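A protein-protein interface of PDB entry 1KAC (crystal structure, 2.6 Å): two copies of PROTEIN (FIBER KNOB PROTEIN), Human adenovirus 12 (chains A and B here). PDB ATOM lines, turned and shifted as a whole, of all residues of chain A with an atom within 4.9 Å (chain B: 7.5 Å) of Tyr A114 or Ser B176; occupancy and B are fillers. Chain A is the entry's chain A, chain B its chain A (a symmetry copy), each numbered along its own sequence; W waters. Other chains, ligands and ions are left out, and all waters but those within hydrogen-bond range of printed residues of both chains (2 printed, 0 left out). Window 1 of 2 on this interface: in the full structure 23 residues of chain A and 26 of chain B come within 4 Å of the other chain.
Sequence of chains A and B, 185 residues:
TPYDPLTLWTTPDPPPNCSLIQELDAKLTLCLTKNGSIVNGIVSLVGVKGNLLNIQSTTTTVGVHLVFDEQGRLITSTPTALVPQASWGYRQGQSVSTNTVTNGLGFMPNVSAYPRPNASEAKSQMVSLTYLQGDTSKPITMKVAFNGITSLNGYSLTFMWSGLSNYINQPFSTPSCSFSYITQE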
ATOM      1  N   PRO A 109     -28.954 -19.603  -4.307  1.00  0.00           N
ATOM      2  CA  PRO A 109     -27.816 -20.522  -4.276  1.00  0.00           C
ATOM      3  C   PRO A 109     -28.177 -21.778  -5.052  1.00  0.00           C
ATOM      4  O   PRO A 109     -29.226 -22.369  -4.820  1.00  0.00           O
ATOM      5  CB  PRO A 109     -27.649 -20.800  -2.783  1.00  0.00           C
ATOM      6  CG  PRO A 109     -28.238 -19.551  -2.144  1.00  0.00           C
ATOM      7  CD  PRO A 109     -29.503 -19.457  -2.954  1.00  0.00           C
ATOM      8  N   ASN A 110     -27.299 -22.189  -5.959  1.00  0.00           N
ATOM      9  CA  ASN A 110     -27.522 -23.366  -6.794  1.00  0.00           C
ATOM     10  C   ASN A 110     -27.758 -24.661  -5.994  1.00  0.00           C
ATOM     11  O   ASN A 110     -26.896 -25.084  -5.217  1.00  0.00           O
ATOM     12  CB  ASN A 110     -26.326 -23.525  -7.732  1.00  0.00           C
ATOM     13  CG  ASN A 110     -26.551 -24.583  -8.795  1.00  0.00           C
ATOM     14  OD1 ASN A 110     -26.636 -25.783  -8.500  1.00  0.00           O
ATOM     15  ND2 ASN A 110     -26.661 -24.141 -10.043  1.00  0.00           N
ATOM     16  N   VAL A 111     -28.919 -25.293  -6.195  1.00  0.00           N
ATOM     17  CA  VAL A 111     -29.243 -26.526  -5.474  1.00  0.00           C
ATOM     18  C   VAL A 111     -28.477 -27.759  -5.924  1.00  0.00           C
ATOM     19  O   VAL A 111     -28.420 -28.750  -5.191  1.00  0.00           O
ATOM     20  CB  VAL A 111     -30.759 -26.864  -5.497  1.00  0.00           C
ATOM     21  CG1 VAL A 111     -31.512 -25.884  -4.634  1.00  0.00           C
ATOM     22  CG2 VAL A 111     -31.289 -26.851  -6.911  1.00  0.00           C
ATOM     23  N   SER A 112     -27.896 -27.723  -7.117  1.00  0.00           N
ATOM     24  CA  SER A 112     -27.113 -28.872  -7.558  1.00  0.00           C
ATOM     25  C   SER A 112     -25.795 -28.798  -6.809  1.00  0.00           C
ATOM     26  O   SER A 112     -25.251 -29.809  -6.373  1.00  0.00           O
ATOM     27  CB  SER A 112     -26.854 -28.825  -9.061  1.00  0.00           C
ATOM     28  OG  SER A 112     -28.070 -28.893  -9.777  1.00  0.00           O
ATOM     29  N   ALA A 113     -25.295 -27.582  -6.648  1.00  0.00           N
ATOM     30  CA  ALA A 113     -24.045 -27.373  -5.938  1.00  0.00           C
ATOM     31  C   ALA A 113     -24.261 -27.453  -4.431  1.00  0.00           C
ATOM     32  O   ALA A 113     -23.388 -27.915  -3.700  1.00  0.00           O
ATOM     33  CB  ALA A 113     -23.461 -26.021  -6.305  1.00  0.00           C
ATOM     34  N   TYR A 114     -25.428 -26.999  -3.975  1.00  0.00           N
ATOM     35  CA  TYR A 114     -25.751 -26.999  -2.546  1.00  0.00           C
ATOM     36  C   TYR A 114     -27.129 -27.636  -2.325  1.00  0.00           C
ATOM     37  O   TYR A 114     -28.112 -26.936  -2.064  1.00  0.00           O
ATOM     38  CB  TYR A 114     -25.760 -25.559  -2.013  1.00  0.00           C
ATOM     39  CG  TYR A 114     -24.631 -24.702  -2.556  1.00  0.00           C
ATOM     40  CD1 TYR A 114     -23.296 -25.033  -2.314  1.00  0.00           C
ATOM     41  CD2 TYR A 114     -24.899 -23.584  -3.351  1.00  0.00           C
ATOM     42  CE1 TYR A 114     -22.254 -24.279  -2.852  1.00  0.00           C
ATOM     43  CE2 TYR A 114     -23.864 -22.819  -3.897  1.00  0.00           C
ATOM     44  CZ  TYR A 114     -22.545 -23.175  -3.646  1.00  0.00           C
ATOM     45  OH  TYR A 114     -21.515 -22.448  -4.212  1.00  0.00           O
ATOM     46  N   PRO A 115     -27.213 -28.979  -2.421  1.00  0.00           N
ATOM     47  CA  PRO A 115     -28.463 -29.727  -2.238  1.00  0.00           C
ATOM     48  C   PRO A 115     -29.134 -29.407  -0.909  1.00  0.00           C
ATOM     49  O   PRO A 115     -28.470 -29.287   0.119  1.00  0.00           O
ATOM     50  CB  PRO A 115     -27.994 -31.179  -2.326  1.00  0.00           C
ATOM     51  CG  PRO A 115     -26.854 -31.076  -3.295  1.00  0.00           C
ATOM     52  CD  PRO A 115     -26.111 -29.920  -2.674  1.00  0.00           C
ATOM     53  N   ARG A 116     -30.454 -29.283  -0.935  1.00  0.00           N
ATOM     54  CA  ARG A 116     -31.211 -28.955   0.266  1.00  0.00           C
ATOM     55  C   ARG A 116     -30.863 -29.796   1.507  1.00  0.00           C
ATOM     56  O   ARG A 116     -30.813 -29.272   2.623  1.00  0.00           O
ATOM     57  CB  ARG A 116     -32.712 -29.005  -0.050  1.00  0.00           C
ATOM     58  CG  ARG A 116     -33.094 -28.038  -1.185  1.00  0.00           C
ATOM     59  CD  ARG A 116     -34.602 -27.839  -1.359  1.00  0.00           C
ATOM     60  NE  ARG A 116     -34.912 -26.863  -2.411  1.00  0.00           N
ATOM     61  CZ  ARG A 116     -34.796 -27.093  -3.720  1.00  0.00           C
ATOM     62  NH1 ARG A 116     -34.374 -28.273  -4.156  1.00  0.00           N
ATOM     63  NH2 ARG A 116     -35.082 -26.139  -4.601  1.00  0.00           N
ATOM     64  N   ALA A 122     -19.469 -29.426   4.020  1.00  0.00           N
ATOM     65  CA  ALA A 122     -18.549 -28.293   3.959  1.00  0.00           C
ATOM     66  C   ALA A 122     -18.765 -27.426   2.722  1.00  0.00           C
ATOM     67  O   ALA A 122     -18.682 -26.203   2.788  1.00  0.00           O
ATOM     68  CB  ALA A 122     -17.115 -28.797   3.991  1.00  0.00           C
ATOM     69  N   LYS A 123     -19.045 -28.071   1.597  1.00  0.00           N
ATOM     70  CA  LYS A 123     -19.261 -27.372   0.339  1.00  0.00           C
ATOM     71  C   LYS A 123     -20.464 -26.428   0.345  1.00  0.00           C
ATOM     72  O   LYS A 123     -20.506 -25.470  -0.428  1.00  0.00           O
ATOM     73  CB  LYS A 123     -19.416 -28.390  -0.788  1.00  0.00           C
ATOM     74  CG  LYS A 123     -19.701 -27.783  -2.138  1.00  0.00           C
ATOM     75  CD  LYS A 123     -19.785 -28.870  -3.175  1.00  0.00           C
ATOM     76  CE  LYS A 123     -20.155 -28.303  -4.527  1.00  0.00           C
ATOM     77  NZ  LYS A 123     -20.427 -29.380  -5.520  1.00  0.00           N
ATOM     78  N   SER A 124     -21.448 -26.695   1.194  1.00  0.00           N
ATOM     79  CA  SER A 124     -22.624 -25.834   1.246  1.00  0.00           C
ATOM     80  C   SER A 124     -22.353 -24.689   2.205  1.00  0.00           C
ATOM     81  O   SER A 124     -23.258 -23.937   2.579  1.00  0.00           O
ATOM     82  CB  SER A 124     -23.850 -26.624   1.707  1.00  0.00           C
ATOM     83  OG  SER A 124     -24.202 -27.610   0.755  1.00  0.00           O
ATOM     84  N   GLN A 125     -21.086 -24.559   2.583  1.00  0.00           N
ATOM     85  CA  GLN A 125     -20.663 -23.530   3.518  1.00  0.00           C
ATOM     86  C   GLN A 125     -19.495 -22.693   3.020  1.00  0.00           C
ATOM     87  O   GLN A 125     -18.635 -23.172   2.280  1.00  0.00           O
ATOM     88  CB  GLN A 125     -20.243 -24.185   4.830  1.00  0.00           C
ATOM     89  CG  GLN A 125     -21.339 -24.936   5.541  1.00  0.00           C
ATOM     90  CD  GLN A 125     -20.799 -25.825   6.635  1.00  0.00           C
ATOM     91  OE1 GLN A 125     -19.988 -25.397   7.459  1.00  0.00           O
ATOM     92  NE2 GLN A 125     -21.255 -27.073   6.657  1.00  0.00           N
ATOM     93  N   MET A 126     -19.487 -21.428   3.413  1.00  0.00           N
ATOM     94  CA  MET A 126     -18.376 -20.546   3.098  1.00  0.00           C
ATOM     95  C   MET A 126     -18.082 -19.946   4.471  1.00  0.00           C
ATOM     96  O   MET A 126     -18.873 -19.163   5.009  1.00  0.00           O
ATOM     97  CB  MET A 126     -18.740 -19.469   2.069  1.00  0.00           C
ATOM     98  CG  MET A 126     -17.524 -18.611   1.723  1.00  0.00           C
ATOM     99  SD  MET A 126     -17.670 -17.513   0.306  1.00  0.00           S
ATOM    100  CE  MET A 126     -17.662 -18.670  -1.061  1.00  0.00           C
ATOM    101  N   VAL A 127     -16.960 -20.368   5.050  1.00  0.00           N
ATOM    102  CA  VAL A 127     -16.571 -19.946   6.389  1.00  0.00           C
ATOM    103  C   VAL A 127     -15.335 -19.067   6.370  1.00  0.00           C
ATOM    104  O   VAL A 127     -14.347 -19.369   5.698  1.00  0.00           O
ATOM    105  CB  VAL A 127     -16.284 -21.175   7.288  1.00  0.00           C
ATOM    106  CG1 VAL A 127     -16.227 -20.756   8.743  1.00  0.00           C
ATOM    107  CG2 VAL A 127     -17.340 -22.246   7.058  1.00  0.00           C
ATOM    108  N   PHE A 146     -25.648 -22.504   2.609  1.00  0.00           N
ATOM    109  CA  PHE A 146     -26.509 -22.390   1.444  1.00  0.00           C
ATOM    110  C   PHE A 146     -27.597 -23.457   1.440  1.00  0.00           C
ATOM    111  O   PHE A 146     -27.310 -24.645   1.552  1.00  0.00           O
ATOM    112  CB  PHE A 146     -25.661 -22.509   0.174  1.00  0.00           C
ATOM    113  CG  PHE A 146     -24.525 -21.527   0.112  1.00  0.00           C
ATOM    114  CD1 PHE A 146     -23.233 -21.959  -0.159  1.00  0.00           C
ATOM    115  CD2 PHE A 146     -24.745 -20.172   0.341  1.00  0.00           C
ATOM    116  CE1 PHE A 146     -22.172 -21.053  -0.196  1.00  0.00           C
ATOM    117  CE2 PHE A 146     -23.695 -19.259   0.306  1.00  0.00           C
ATOM    118  CZ  PHE A 146     -22.404 -19.698   0.037  1.00  0.00           C
ATOM    119  N   ASN A 147     -28.844 -23.019   1.312  1.00  0.00           N
ATOM    120  CA  ASN A 147     -29.994 -23.913   1.262  1.00  0.00           C
ATOM    121  C   ASN A 147     -30.095 -24.931   2.393  1.00  0.00           C
ATOM    122  O   ASN A 147     -30.514 -26.070   2.182  1.00  0.00           O
ATOM    123  CB  ASN A 147     -30.028 -24.641  -0.080  1.00  0.00           C
ATOM    124  CG  ASN A 147     -30.177 -23.692  -1.253  1.00  0.00           C
ATOM    125  OD1 ASN A 147     -31.020 -22.789  -1.233  1.00  0.00           O
ATOM    126  ND2 ASN A 147     -29.378 -23.903  -2.295  1.00  0.00           N
ATOM    127  N   TYR A 181     -21.619 -17.117  -3.850  1.00  0.00           N
ATOM    128  CA  TYR A 181     -22.095 -18.463  -4.115  1.00  0.00           C
ATOM    129  C   TYR A 181     -22.507 -18.631  -5.564  1.00  0.00           C
ATOM    130  O   TYR A 181     -22.751 -17.641  -6.271  1.00  0.00           O
ATOM    131  CB  TYR A 181     -23.257 -18.803  -3.174  1.00  0.00           C
ATOM    132  CG  TYR A 181     -24.378 -17.784  -3.171  1.00  0.00           C
ATOM    133  CD1 TYR A 181     -25.372 -17.794  -4.150  1.00  0.00           C
ATOM    134  CD2 TYR A 181     -24.420 -16.783  -2.203  1.00  0.00           C
ATOM    135  CE1 TYR A 181     -26.381 -16.828  -4.160  1.00  0.00           C
ATOM    136  CE2 TYR A 181     -25.416 -15.817  -2.204  1.00  0.00           C
ATOM    137  CZ  TYR A 181     -26.393 -15.843  -3.183  1.00  0.00           C
ATOM    138  OH  TYR A 181     -27.370 -14.878  -3.172  1.00  0.00           O
ATOM    139  N   ILE A 182     -22.547 -19.888  -6.008  1.00  0.00           N
ATOM    140  CA  ILE A 182     -22.933 -20.206  -7.373  1.00  0.00           C
ATOM    141  C   ILE A 182     -24.434 -20.031  -7.425  1.00  0.00           C
ATOM    142  O   ILE A 182     -25.127 -20.378  -6.479  1.00  0.00           O
ATOM    143  CB  ILE A 182     -22.553 -21.646  -7.744  1.00  0.00           C
ATOM    144  CG1 ILE A 182     -21.039 -21.815  -7.617  1.00  0.00           C
ATOM    145  CG2 ILE A 182     -23.003 -21.946  -9.166  1.00  0.00           C
ATOM    146  CD1 ILE A 182     -20.547 -23.198  -7.916  1.00  0.00           C
ATOM    147  N   PRO B  12     -22.037 -27.404 -11.318  1.00  0.00           N
ATOM    148  CA  PRO B  12     -22.174 -27.358  -9.859  1.00  0.00           C
ATOM    149  C   PRO B  12     -21.925 -28.643  -9.070  1.00  0.00           C
ATOM    150  O   PRO B  12     -21.445 -28.592  -7.941  1.00  0.00           O
ATOM    151  CB  PRO B  12     -23.596 -26.840  -9.686  1.00  0.00           C
ATOM    152  CG  PRO B  12     -24.301 -27.492 -10.854  1.00  0.00           C
ATOM    153  CD  PRO B  12     -23.334 -27.122 -11.954  1.00  0.00           C
ATOM    154  N   ASP B  13     -22.242 -29.788  -9.668  1.00  0.00           N
ATOM    155  CA  ASP B  13     -22.107 -31.078  -8.984  1.00  0.00           C
ATOM    156  C   ASP B  13     -21.320 -32.127  -9.761  1.00  0.00           C
ATOM    157  O   ASP B  13     -21.830 -33.190 -10.099  1.00  0.00           O
ATOM    158  CB  ASP B  13     -23.504 -31.618  -8.691  1.00  0.00           C
ATOM    159  CG  ASP B  13     -24.286 -31.907  -9.957  1.00  0.00           C
ATOM    160  OD1 ASP B  13     -24.335 -31.018 -10.839  1.00  0.00           O
ATOM    161  OD2 ASP B  13     -24.853 -33.019 -10.072  1.00  0.00           O
ATOM    162  N   THR B  29     -14.953 -28.782  -7.460  1.00  0.00           N
ATOM    163  CA  THR B  29     -15.999 -27.935  -8.001  1.00  0.00           C
ATOM    164  C   THR B  29     -15.377 -26.553  -8.106  1.00  0.00           C
ATOM    165  O   THR B  29     -14.938 -25.984  -7.105  1.00  0.00           O
ATOM    166  CB  THR B  29     -17.216 -27.858  -7.077  1.00  0.00           C
ATOM    167  OG1 THR B  29     -17.691 -29.177  -6.812  1.00  0.00           O
ATOM    168  CG2 THR B  29     -18.327 -27.065  -7.737  1.00  0.00           C
ATOM    169  N   CYS B  31     -15.843 -22.641 -10.083  1.00  0.00           N
ATOM    170  CA  CYS B  31     -16.614 -21.740 -10.911  1.00  0.00           C
ATOM    171  C   CYS B  31     -15.899 -20.393 -11.002  1.00  0.00           C
ATOM    172  O   CYS B  31     -15.528 -19.806  -9.989  1.00  0.00           O
ATOM    173  CB  CYS B  31     -18.015 -21.566 -10.331  1.00  0.00           C
ATOM    174  SG  CYS B  31     -19.079 -20.515 -11.342  1.00  0.00           S
ATOM    175  N   GLY B  41     -13.967 -16.078  -8.167  1.00  0.00           N
ATOM    176  CA  GLY B  41     -13.923 -17.521  -8.213  1.00  0.00           C
ATOM    177  C   GLY B  41     -14.329 -18.167  -6.910  1.00  0.00           C
ATOM    178  O   GLY B  41     -14.159 -17.593  -5.837  1.00  0.00           O
ATOM    179  N   ILE B  42     -14.897 -19.361  -7.010  1.00  0.00           N
ATOM    180  CA  ILE B  42     -15.278 -20.123  -5.833  1.00  0.00           C
ATOM    181  C   ILE B  42     -14.810 -21.557  -6.080  1.00  0.00           C
ATOM    182  O   ILE B  42     -15.216 -22.197  -7.048  1.00  0.00           O
ATOM    183  CB  ILE B  42     -16.802 -20.098  -5.590  1.00  0.00           C
ATOM    184  CG1 ILE B  42     -17.271 -18.651  -5.394  1.00  0.00           C
ATOM    185  CG2 ILE B  42     -17.138 -20.943  -4.369  1.00  0.00           C
ATOM    186  CD1 ILE B  42     -18.755 -18.506  -5.156  1.00  0.00           C
ATOM    187  N   VAL B  43     -13.926 -22.049  -5.223  1.00  0.00           N
ATOM    188  CA  VAL B  43     -13.417 -23.400  -5.376  1.00  0.00           C
ATOM    189  C   VAL B  43     -13.766 -24.255  -4.163  1.00  0.00           C
ATOM    190  O   VAL B  43     -13.942 -23.749  -3.054  1.00  0.00           O
ATOM    191  CB  VAL B  43     -11.886 -23.399  -5.571  1.00  0.00           C
ATOM    192  CG1 VAL B  43     -11.200 -22.885  -4.316  1.00  0.00           C
ATOM    193  CG2 VAL B  43     -11.404 -24.791  -5.921  1.00  0.00           C
ATOM    194  N   SER B  44     -13.863 -25.558  -4.393  1.00  0.00           N
ATOM    195  CA  SER B  44     -14.182 -26.508  -3.340  1.00  0.00           C
ATOM    196  C   SER B  44     -13.578 -27.860  -3.720  1.00  0.00           C
ATOM    197  O   SER B  44     -13.680 -28.291  -4.871  1.00  0.00           O
ATOM    198  CB  SER B  44     -15.701 -26.620  -3.199  1.00  0.00           C
ATOM    199  OG  SER B  44     -16.046 -27.465  -2.123  1.00  0.00           O
ATOM    200  N   LEU B  45     -12.945 -28.526  -2.762  1.00  0.00           N
ATOM    201  CA  LEU B  45     -12.324 -29.821  -3.024  1.00  0.00           C
ATOM    202  C   LEU B  45     -12.675 -30.837  -1.944  1.00  0.00           C
ATOM    203  O   LEU B  45     -12.660 -30.526  -0.756  1.00  0.00           O
ATOM    204  CB  LEU B  45     -10.799 -29.670  -3.100  1.00  0.00           C
ATOM    205  CG  LEU B  45      -9.981 -30.926  -3.425  1.00  0.00           C
ATOM    206  CD1 LEU B  45     -10.360 -31.442  -4.801  1.00  0.00           C
ATOM    207  CD2 LEU B  45      -8.495 -30.606  -3.377  1.00  0.00           C
ATOM    208  N   THR B 130      -9.315 -20.556   6.468  1.00  0.00           N
ATOM    209  CA  THR B 130     -10.607 -21.210   6.301  1.00  0.00           C
ATOM    210  C   THR B 130     -10.660 -22.432   7.217  1.00  0.00           C
ATOM    211  O   THR B 130      -9.806 -22.584   8.092  1.00  0.00           O
ATOM    212  CB  THR B 130     -10.882 -21.593   4.821  1.00  0.00           C
ATOM    213  OG1 THR B 130     -12.256 -21.981   4.691  1.00  0.00           O
ATOM    214  CG2 THR B 130      -9.980 -22.738   4.368  1.00  0.00           C
ATOM    215  N   TYR B 131     -11.650 -23.300   7.040  1.00  0.00           N
ATOM    216  CA  TYR B 131     -11.761 -24.449   7.933  1.00  0.00           C
ATOM    217  C   TYR B 131     -12.076 -25.791   7.292  1.00  0.00           C
ATOM    218  O   TYR B 131     -13.002 -25.909   6.491  1.00  0.00           O
ATOM    219  CB  TYR B 131     -12.811 -24.156   9.015  1.00  0.00           C
ATOM    220  CG  TYR B 131     -12.595 -22.836   9.710  1.00  0.00           C
ATOM    221  CD1 TYR B 131     -12.990 -21.641   9.109  1.00  0.00           C
ATOM    222  CD2 TYR B 131     -11.914 -22.770  10.928  1.00  0.00           C
ATOM    223  CE1 TYR B 131     -12.708 -20.408   9.702  1.00  0.00           C
ATOM    224  CE2 TYR B 131     -11.628 -21.546  11.528  1.00  0.00           C
ATOM    225  CZ  TYR B 131     -12.026 -20.367  10.910  1.00  0.00           C
ATOM    226  OH  TYR B 131     -11.738 -19.149  11.493  1.00  0.00           O
ATOM    227  N   GLY B 134     -15.368 -27.313   7.239  1.00  0.00           N
ATOM    228  CA  GLY B 134     -16.189 -26.130   7.417  1.00  0.00           C
ATOM    229  C   GLY B 134     -16.368 -25.967   8.918  1.00  0.00           C
ATOM    230  O   GLY B 134     -17.102 -25.106   9.392  1.00  0.00           O
ATOM    231  N   MET B 142      -5.704 -21.385   2.927  1.00  0.00           N
ATOM    232  CA  MET B 142      -5.844 -21.647   1.506  1.00  0.00           C
ATOM    233  C   MET B 142      -5.021 -20.612   0.766  1.00  0.00           C
ATOM    234  O   MET B 142      -5.204 -19.406   0.951  1.00  0.00           O
ATOM    235  CB  MET B 142      -7.283 -21.546   1.006  1.00  0.00           C
ATOM    236  CG  MET B 142      -7.316 -21.774  -0.504  1.00  0.00           C
ATOM    237  SD  MET B 142      -8.889 -21.722  -1.336  1.00  0.00           S
ATOM    238  CE  MET B 142      -9.344 -19.986  -1.158  1.00  0.00           C
ATOM    239  N   TRP B 161      -4.128 -26.147   0.230  1.00  0.00           N
ATOM    240  CA  TRP B 161      -4.794 -26.133   1.523  1.00  0.00           C
ATOM    241  C   TRP B 161      -3.761 -26.718   2.480  1.00  0.00           C
ATOM    242  O   TRP B 161      -3.462 -27.914   2.434  1.00  0.00           O
ATOM    243  CB  TRP B 161      -6.063 -26.980   1.477  1.00  0.00           C
ATOM    244  CG  TRP B 161      -7.200 -26.261   0.849  1.00  0.00           C
ATOM    245  CD1 TRP B 161      -8.017 -25.343   1.444  1.00  0.00           C
ATOM    246  CD2 TRP B 161      -7.606 -26.325  -0.522  1.00  0.00           C
ATOM    247  NE1 TRP B 161      -8.905 -24.830   0.531  1.00  0.00           N
ATOM    248  CE2 TRP B 161      -8.672 -25.414  -0.684  1.00  0.00           C
ATOM    249  CE3 TRP B 161      -7.165 -27.058  -1.628  1.00  0.00           C
ATOM    250  CZ2 TRP B 161      -9.309 -25.224  -1.907  1.00  0.00           C
ATOM    251  CZ3 TRP B 161      -7.796 -26.867  -2.842  1.00  0.00           C
ATOM    252  CH2 TRP B 161      -8.857 -25.956  -2.972  1.00  0.00           C
ATOM    253  N   THR B 174     -12.990 -29.300   1.909  1.00  0.00           N
ATOM    254  CA  THR B 174     -12.987 -27.854   2.126  1.00  0.00           C
ATOM    255  C   THR B 174     -14.375 -27.256   1.925  1.00  0.00           C
ATOM    256  O   THR B 174     -15.254 -27.880   1.329  1.00  0.00           O
ATOM    257  CB  THR B 174     -12.076 -27.119   1.124  1.00  0.00           C
ATOM    258  OG1 THR B 174     -12.729 -27.071  -0.151  1.00  0.00           O
ATOM    259  CG2 THR B 174     -10.744 -27.837   0.974  1.00  0.00           C
ATOM    260  N   PRO B 175     -14.594 -26.040   2.443  1.00  0.00           N
ATOM    261  CA  PRO B 175     -15.869 -25.333   2.310  1.00  0.00           C
ATOM    262  C   PRO B 175     -15.756 -24.676   0.936  1.00  0.00           C
ATOM    263  O   PRO B 175     -14.714 -24.789   0.295  1.00  0.00           O
ATOM    264  CB  PRO B 175     -15.791 -24.273   3.422  1.00  0.00           C
ATOM    265  CG  PRO B 175     -14.615 -24.772   4.328  1.00  0.00           C
ATOM    266  CD  PRO B 175     -13.673 -25.247   3.273  1.00  0.00           C
ATOM    267  N   SER B 176     -16.806 -24.015   0.470  1.00  0.00           N
ATOM    268  CA  SER B 176     -16.698 -23.316  -0.801  1.00  0.00           C
ATOM    269  C   SER B 176     -15.814 -22.116  -0.472  1.00  0.00           C
ATOM    270  O   SER B 176     -16.185 -21.286   0.363  1.00  0.00           O
ATOM    271  CB  SER B 176     -18.065 -22.838  -1.291  1.00  0.00           C
ATOM    272  OG  SER B 176     -18.829 -23.918  -1.775  1.00  0.00           O
ATOM    273  N   CYS B 177     -14.646 -22.038  -1.107  1.00  0.00           N
ATOM    274  CA  CYS B 177     -13.699 -20.955  -0.851  1.00  0.00           C
ATOM    275  C   CYS B 177     -13.641 -19.946  -1.982  1.00  0.00           C
ATOM    276  O   CYS B 177     -13.476 -20.298  -3.150  1.00  0.00           O
ATOM    277  CB  CYS B 177     -12.301 -21.520  -0.611  1.00  0.00           C
ATOM    278  SG  CYS B 177     -12.223 -22.748   0.709  1.00  0.00           S
ATOM    279  N   SER B 178     -13.765 -18.679  -1.617  1.00  0.00           N
ATOM    280  CA  SER B 178     -13.740 -17.602  -2.583  1.00  0.00           C
ATOM    281  C   SER B 178     -12.336 -17.070  -2.820  1.00  0.00           C
ATOM    282  O   SER B 178     -11.440 -17.211  -1.982  1.00  0.00           O
ATOM    283  CB  SER B 178     -14.641 -16.465  -2.104  1.00  0.00           C
ATOM    284  OG  SER B 178     -14.253 -16.026  -0.809  1.00  0.00           O
HETATM  285  O   HOH W   1     -14.059 -18.303   1.123  1.00  0.00           O
HETATM  286  O   HOH W   2     -15.146 -21.170   2.870  1.00  0.00           O
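Among the printed residues, pairs that only touch across the chains: Asn A110 with Pro B12, Ser A112 with Pro B12, Ser A112 with Asp B13, Ala A113 with Pro B12, Tyr A114 with Ser B176, Ala A122 with Gly B134, Ala A122 with Thr B174, Ala A122 with Pro B175, Ala A122 with Ser B176, Lys A123 with Ser B44, Lys A123 with Thr B174, Gln A125 with Pro B175, Met A126 with Ser B176, Met A126 with Ser B178, Val A127 with Tyr B131, Val A127 with Gly B134, Tyr A181 with Ile B42 and Ile A182 with Cys B31.
Water W2 lies within hydrogen-bond range of O of Ser B176 (2.7 Å) and N of Val A127 (2.9 Å). Water W1 lies within hydrogen-bond range of the backbone NH of Ser B178 and the side-chain sulfur of Met A126.
Of the 19 printed residues of chain B, 13 touch a printed residue of chain A. Hydrophobic or aromatic side chains of chain B that line the printed part of chain A: Pro B12, Ile B42, Tyr B131 and Pro B175. Along chain B the printed residues that touch a printed residue of chain A span positions 12 to 178. Printed residues of chain A that touch a printed residue of chain B: Asn A110, Ser A112, Ala A113, Tyr A114, Ala A122, Lys A123, Gln A125, Met A126, Val A127, Tyr A181 and Ile A182. Hydrophobic or aromatic side chains of chain A within 4 Å of the printed part of chain B: Ala A113, Tyr A114, Ala A122, Met A126, Val A127 and Ile A182. Among the printed residues, no Asp or Glu carboxylate lies within 4 Å of a Lys or Arg side-chain nitrogen of the other chain.
The backbone NH (N) of Asn A110 is in hydrogen-bond range of the backbone carbonyl oxygen (O) of Ile A182 (2.9 Å). N of Ile A182 is in hydrogen-bond range of OH of Tyr A114, 3.3 Å away. The backbone carbonyl oxygen (O) of Ser B44 sits at hydrogen-bond distance from the backbone NH (N) of Thr B29 (2.9 Å). The side-chain amide oxygen of Asn A110 is in hydrogen-bond range of the backbone NH of Ala A113, 2.9 Å away. O of Pro B175 lies within hydrogen-bond range of SG of Cys B177, at 3.2 Å. The backbone carbonyl oxygen (O) of Cys B31 is in hydrogen-bond range of the backbone NH (N) of Ile B42, at 3.1 Å.
The side-chain hydroxyl (OG1) of Thr B130 sits at hydrogen-bond distance from the backbone carbonyl oxygen (O) of Val A127, 3.5 Å away. The side-chain amino group (NZ) of Lys A123 sits at hydrogen-bond distance from the backbone carbonyl oxygen (O) of Pro B12. O of Gln A125 sits at hydrogen-bond distance from N of Ser B176 (2.7 Å). The backbone carbonyl oxygen (O) of Lys A123 sits at hydrogen-bond distance from the side-chain hydroxyl (OG) of Ser B176 (2.7 Å). The side-chain amide oxygen (OE1) of Gln A125 lies close to the backbone carbonyl oxygen (O) of Gly B134 (3.5 Å). The side-chain hydroxyl (OG1) of Thr B29 is in hydrogen-bond range of the side-chain amino group (NZ) of Lys A123.
No position is printed for both chains.
Ala A113 touches one residue of chain B. Tyr A114 touches one residue of chain B. Arg A116 touches none of the printed residues of chain B. Printed residues of chain B within 4 Å of Lys A123: Pro B12 (2.7 Å), Thr B29 (3.0 Å), Ser B44 (3.7 Å), Thr B174 (3.8 Å) and Ser B176 (2.7 Å). Printed residues of chain B within 4 Å of Gln A125: Gly B134 (3.5 Å), Pro B175 (3.3 Å) and Ser B176 (2.7 Å). Printed residues of chain B within 4 Å of Met A126: Ser B176 and Ser B178. Of the printed residues of chain A, Gly B134 touches Ala A122 (3.98 Å), Gln A125 (3.5 Å) and Val A127 (3.7 Å). Of the printed residues of chain A, Pro B175 touches Ala A122 (3.0 Å) and Gln A125 (3.3 Å). Ser B176 touches five residues of chain A. The nearest residue of chain B that does not touch Tyr A114 is Ile B42 (4.6 Å). The nearest residue of chain A that does not touch Ser B176 is Phe A146 (4.6 Å).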
